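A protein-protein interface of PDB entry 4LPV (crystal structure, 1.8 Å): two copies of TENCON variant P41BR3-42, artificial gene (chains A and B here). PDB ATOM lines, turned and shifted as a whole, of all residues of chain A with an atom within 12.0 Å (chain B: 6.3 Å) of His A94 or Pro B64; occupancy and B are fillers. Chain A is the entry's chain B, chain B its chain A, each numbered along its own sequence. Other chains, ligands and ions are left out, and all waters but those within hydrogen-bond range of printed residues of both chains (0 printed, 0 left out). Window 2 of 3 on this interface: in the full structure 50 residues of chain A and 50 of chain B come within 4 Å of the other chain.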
ATOM      1  N   PHE A  89      12.672  -5.396   6.299  1.00  0.00           N
ATOM      2  CA  PHE A  89      12.351  -6.776   5.963  1.00  0.00           C
ATOM      3  C   PHE A  89      13.172  -7.680   6.874  1.00  0.00           C
ATOM      4  O   PHE A  89      14.245  -7.294   7.332  1.00  0.00           O
ATOM      5  CB  PHE A  89      12.657  -7.091   4.489  1.00  0.00           C
ATOM      6  CG  PHE A  89      12.019  -6.138   3.515  1.00  0.00           C
ATOM      7  CD1 PHE A  89      10.673  -6.253   3.189  1.00  0.00           C
ATOM      8  CD2 PHE A  89      12.759  -5.115   2.934  1.00  0.00           C
ATOM      9  CE1 PHE A  89      10.077  -5.368   2.302  1.00  0.00           C
ATOM     10  CE2 PHE A  89      12.172  -4.229   2.046  1.00  0.00           C
ATOM     11  CZ  PHE A  89      10.831  -4.355   1.727  1.00  0.00           C
ATOM     12  N   THR A  90      12.660  -8.876   7.146  1.00  0.00           N
ATOM     13  CA  THR A  90      13.384  -9.848   7.958  1.00  0.00           C
ATOM     14  C   THR A  90      13.708 -11.086   7.125  1.00  0.00           C
ATOM     15  O   THR A  90      12.845 -11.632   6.436  1.00  0.00           O
ATOM     16  CB  THR A  90      12.598 -10.214   9.240  1.00  0.00           C
ATOM     17  OG1 THR A  90      12.227  -9.012   9.935  1.00  0.00           O
ATOM     18  CG2 THR A  90      13.446 -11.086  10.165  1.00  0.00           C
ATOM     19  N   THR A  91      14.966 -11.503   7.154  1.00  0.00           N
ATOM     20  CA  THR A  91      15.384 -12.694   6.425  1.00  0.00           C
ATOM     21  C   THR A  91      14.791 -13.928   7.108  1.00  0.00           C
ATOM     22  O   THR A  91      14.431 -13.876   8.284  1.00  0.00           O
ATOM     23  CB  THR A  91      16.920 -12.816   6.368  1.00  0.00           C
ATOM     24  OG1 THR A  91      17.445 -12.762   7.698  1.00  0.00           O
ATOM     25  CG2 THR A  91      17.528 -11.666   5.562  1.00  0.00           C
ATOM     26  N   GLY A  92      14.695 -15.028   6.370  1.00  0.00           N
ATOM     27  CA  GLY A  92      14.114 -16.254   6.896  1.00  0.00           C
ATOM     28  C   GLY A  92      14.993 -16.992   7.894  1.00  0.00           C
ATOM     29  O   GLY A  92      16.217 -16.795   7.951  1.00  0.00           O
ATOM     30  N   GLY A  93      14.369 -17.853   8.694  1.00  0.00           N
ATOM     31  CA  GLY A  93      15.114 -18.678   9.626  1.00  0.00           C
ATOM     32  C   GLY A  93      15.265 -18.096  11.016  1.00  0.00           C
ATOM     33  O   GLY A  93      14.613 -17.118  11.383  1.00  0.00           O
ATOM     34  N   HIS A  94      16.143 -18.713  11.796  1.00  0.00           N
ATOM     35  CA  HIS A  94      16.315 -18.350  13.195  1.00  0.00           C
ATOM     36  C   HIS A  94      17.523 -17.459  13.424  1.00  0.00           C
ATOM     37  O   HIS A  94      18.621 -17.754  12.953  1.00  0.00           O
ATOM     38  CB  HIS A  94      16.416 -19.614  14.048  1.00  0.00           C
ATOM     39  CG  HIS A  94      15.137 -20.382  14.124  1.00  0.00           C
ATOM     40  ND1 HIS A  94      14.099 -19.996  14.940  1.00  0.00           N
ATOM     41  CD2 HIS A  94      14.711 -21.483  13.461  1.00  0.00           C
ATOM     42  CE1 HIS A  94      13.098 -20.843  14.803  1.00  0.00           C
ATOM     43  NE2 HIS A  94      13.438 -21.752  13.906  1.00  0.00           N
ATOM     44  N   HIS A  95      17.309 -16.376  14.166  1.00  0.00           N
ATOM     45  CA  HIS A  95      18.355 -15.401  14.458  1.00  0.00           C
ATOM     46  C   HIS A  95      19.505 -16.008  15.264  1.00  0.00           C
ATOM     47  O   HIS A  95      19.326 -17.006  15.966  1.00  0.00           O
ATOM     48  CB  HIS A  95      17.763 -14.187  15.196  1.00  0.00           C
ATOM     49  N   THR B  14      14.934 -15.558   1.632  1.00  0.00           N
ATOM     50  CA  THR B  14      15.528 -16.806   2.106  1.00  0.00           C
ATOM     51  C   THR B  14      16.249 -16.550   3.419  1.00  0.00           C
ATOM     52  O   THR B  14      16.106 -15.476   4.013  1.00  0.00           O
ATOM     53  CB  THR B  14      16.482 -17.476   1.076  1.00  0.00           C
ATOM     54  OG1 THR B  14      17.751 -16.804   1.047  1.00  0.00           O
ATOM     55  CG2 THR B  14      15.863 -17.498  -0.317  1.00  0.00           C
ATOM     56  N   GLU B  15      17.015 -17.533   3.879  1.00  0.00           N
ATOM     57  CA  GLU B  15      17.721 -17.392   5.150  1.00  0.00           C
ATOM     58  C   GLU B  15      18.949 -16.480   5.060  1.00  0.00           C
ATOM     59  O   GLU B  15      19.542 -16.133   6.071  1.00  0.00           O
ATOM     60  CB  GLU B  15      18.086 -18.765   5.720  1.00  0.00           C
ATOM     61  CG  GLU B  15      16.872 -19.554   6.172  1.00  0.00           C
ATOM     62  CD  GLU B  15      17.175 -21.013   6.398  1.00  0.00           C
ATOM     63  OE1 GLU B  15      18.176 -21.313   7.082  1.00  0.00           O
ATOM     64  OE2 GLU B  15      16.417 -21.861   5.882  1.00  0.00           O
ATOM     65  N   ASP B  16      19.323 -16.091   3.847  1.00  0.00           N
ATOM     66  CA  ASP B  16      20.418 -15.142   3.674  1.00  0.00           C
ATOM     67  C   ASP B  16      20.235 -14.216   2.472  1.00  0.00           C
ATOM     68  O   ASP B  16      21.213 -13.715   1.912  1.00  0.00           O
ATOM     69  CB  ASP B  16      21.769 -15.863   3.597  1.00  0.00           C
ATOM     70  CG  ASP B  16      21.866 -16.820   2.427  1.00  0.00           C
ATOM     71  OD1 ASP B  16      20.972 -16.825   1.556  1.00  0.00           O
ATOM     72  OD2 ASP B  16      22.861 -17.572   2.374  1.00  0.00           O
ATOM     73  N   LEU B  62      23.227 -12.141   3.478  1.00  0.00           N
ATOM     74  CA  LEU B  62      22.682 -11.594   4.714  1.00  0.00           C
ATOM     75  C   LEU B  62      22.679 -12.631   5.848  1.00  0.00           C
ATOM     76  O   LEU B  62      23.074 -13.783   5.663  1.00  0.00           O
ATOM     77  CB  LEU B  62      21.261 -11.066   4.471  1.00  0.00           C
ATOM     78  CG  LEU B  62      21.048 -10.069   3.324  1.00  0.00           C
ATOM     79  CD1 LEU B  62      19.574  -9.774   3.119  1.00  0.00           C
ATOM     80  CD2 LEU B  62      21.839  -8.771   3.541  1.00  0.00           C
ATOM     81  N   LYS B  63      22.228 -12.204   7.019  1.00  0.00           N
ATOM     82  CA  LYS B  63      22.135 -13.070   8.186  1.00  0.00           C
ATOM     83  C   LYS B  63      20.713 -13.600   8.355  1.00  0.00           C
ATOM     84  O   LYS B  63      19.758 -12.942   7.941  1.00  0.00           O
ATOM     85  CB  LYS B  63      22.557 -12.304   9.435  1.00  0.00           C
ATOM     86  CG  LYS B  63      24.043 -12.000   9.493  1.00  0.00           C
ATOM     87  CD  LYS B  63      24.313 -10.875  10.467  1.00  0.00           C
ATOM     88  CE  LYS B  63      23.409 -10.984  11.680  1.00  0.00           C
ATOM     89  NZ  LYS B  63      23.838 -10.075  12.781  1.00  0.00           N
ATOM     90  N   PRO B  64      20.571 -14.799   8.959  1.00  0.00           N
ATOM     91  CA  PRO B  64      19.258 -15.433   9.163  1.00  0.00           C
ATOM     92  C   PRO B  64      18.466 -14.759  10.286  1.00  0.00           C
ATOM     93  O   PRO B  64      19.087 -14.278  11.240  1.00  0.00           O
ATOM     94  CB  PRO B  64      19.616 -16.876   9.553  1.00  0.00           C
ATOM     95  CG  PRO B  64      21.091 -17.029   9.261  1.00  0.00           C
ATOM     96  CD  PRO B  64      21.673 -15.669   9.410  1.00  0.00           C
ATOM     97  N   GLY B  65      17.136 -14.724  10.162  1.00  0.00           N
ATOM     98  CA  GLY B  65      16.249 -14.170  11.176  1.00  0.00           C
ATOM     99  C   GLY B  65      16.649 -12.778  11.625  1.00  0.00           C
ATOM    100  O   GLY B  65      16.570 -12.432  12.810  1.00  0.00           O
ATOM    101  N   THR B  66      17.083 -11.974  10.662  1.00  0.00           N
ATOM    102  CA  THR B  66      17.607 -10.646  10.943  1.00  0.00           C
ATOM    103  C   THR B  66      16.841  -9.589  10.147  1.00  0.00           C
ATOM    104  O   THR B  66      16.604  -9.747   8.945  1.00  0.00           O
ATOM    105  CB  THR B  66      19.124 -10.583  10.625  1.00  0.00           C
ATOM    106  OG1 THR B  66      19.831 -11.451  11.523  1.00  0.00           O
ATOM    107  CG2 THR B  66      19.657  -9.166  10.764  1.00  0.00           C
ATOM    108  N   TYR B  68      16.491  -6.067   8.290  1.00  0.00           N
ATOM    109  CA  TYR B  68      17.306  -5.086   7.570  1.00  0.00           C
ATOM    110  C   TYR B  68      16.444  -3.879   7.202  1.00  0.00           C
ATOM    111  O   TYR B  68      15.280  -4.039   6.836  1.00  0.00           O
ATOM    112  CB  TYR B  68      17.914  -5.711   6.302  1.00  0.00           C
ATOM    113  CG  TYR B  68      19.006  -6.707   6.588  1.00  0.00           C
ATOM    114  CD1 TYR B  68      18.706  -8.026   6.931  1.00  0.00           C
ATOM    115  CD2 TYR B  68      20.344  -6.329   6.536  1.00  0.00           C
ATOM    116  CE1 TYR B  68      19.710  -8.939   7.207  1.00  0.00           C
ATOM    117  CE2 TYR B  68      21.351  -7.232   6.807  1.00  0.00           C
ATOM    118  CZ  TYR B  68      21.030  -8.537   7.149  1.00  0.00           C
ATOM    119  OH  TYR B  68      22.036  -9.432   7.417  1.00  0.00           O
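N of Thr A91 lies within hydrogen-bond range of O of Thr B66.
O of Thr B14 lies within hydrogen-bond range of N of Gly A92 (2.8 Å).
The side-chain hydroxyl (OG1) of Thr A91 lies close to the backbone carbonyl oxygen (O) of Lys B63, at 2.3 Å.
O of Phe A89 lies within hydrogen-bond range of N of Tyr B68.
N of Gly B65 sits at hydrogen-bond distance from OG1 of Thr A91 (3.2 Å).
The backbone NH of Gly B65 is in hydrogen-bond range of the backbone carbonyl oxygen of Gly A92, at 3.2 Å.
Thr B66 touches Phe A89.
Gly B65 touches Thr A90 (C to CG2, 3.9 Å).
OG1 of Thr A91 touches C of Pro B64, 3.4 Å away.
Tyr B68 touches Thr A91.
Gly A92 touches Glu B15 (O to CA, 3.2 Å).
Gly A92 touches Pro B64 (O to CA, 3.5 Å).
Glu B15 touches Gly A93 (CG to N, 3.9 Å).
O of Gly A93 touches CA of Gly B65, at 3.4 Å.
Pro B64 touches His A94.
His A95 touches Gly B65 (CB to O, 3.2 Å).
Of chain B, only Pro B64 comes within 4 Å of His A94.
Pro B64 touches just these residues of chain A: Thr A91, Gly A92, His A94 and His A95.
Glu B15 touches two residues of chain A.
Asp B16 touches none of the printed residues of chain A.
Of chain A, only Thr A91 comes within 4 Å of Lys B63.
Gly B65 touches five residues of chain A.
Of chain A, only Phe A89, Thr A90 and Thr A91 come within 4 Å of Thr B66.
Of the printed residues of chain B, Thr A91 touches Thr B14 (3.6 Å), Leu B62 (3.7 Å), Lys B63 (2.3 Å), Pro B64 (3.4 Å), Gly B65 (3.2 Å), Thr B66 (3.0 Å) and Tyr B68 (3.9 Å).
Of the printed residues of chain B, Phe A89 touches Thr B66 (3.8 Å) and Tyr B68 (2.7 Å).
No position is printed for both chains.
Of the 9 printed residues of chain B, 8 touch a printed residue of chain A.
Along chain B the printed residues that touch a printed residue of chain A span positions 14 to 68.
Printed residues of chain A that touch a printed residue of chain B: Phe A89, Thr A90, Thr A91, Gly A92, Gly A93, His A94 and His A95.
Hydrophobic or aromatic side chains of chain A that line the printed part of chain B: His A95.
Among the printed residues, 20 pairs touch across the chains.
The side-chain hydroxyl (OG1) of Thr B14 is in hydrogen-bond range of the side-chain carboxylate (OD1) of Asp B16 (3.3 Å).
The side-chain hydroxyl (OG1) of Thr B66 sits at hydrogen-bond distance from the backbone carbonyl oxygen (O) of Pro B64.
OH of Tyr B68 lies within hydrogen-bond range of N of Lys B63 (2.8 Å).
O of Asp B16 is in hydrogen-bond range of N of Leu B62.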
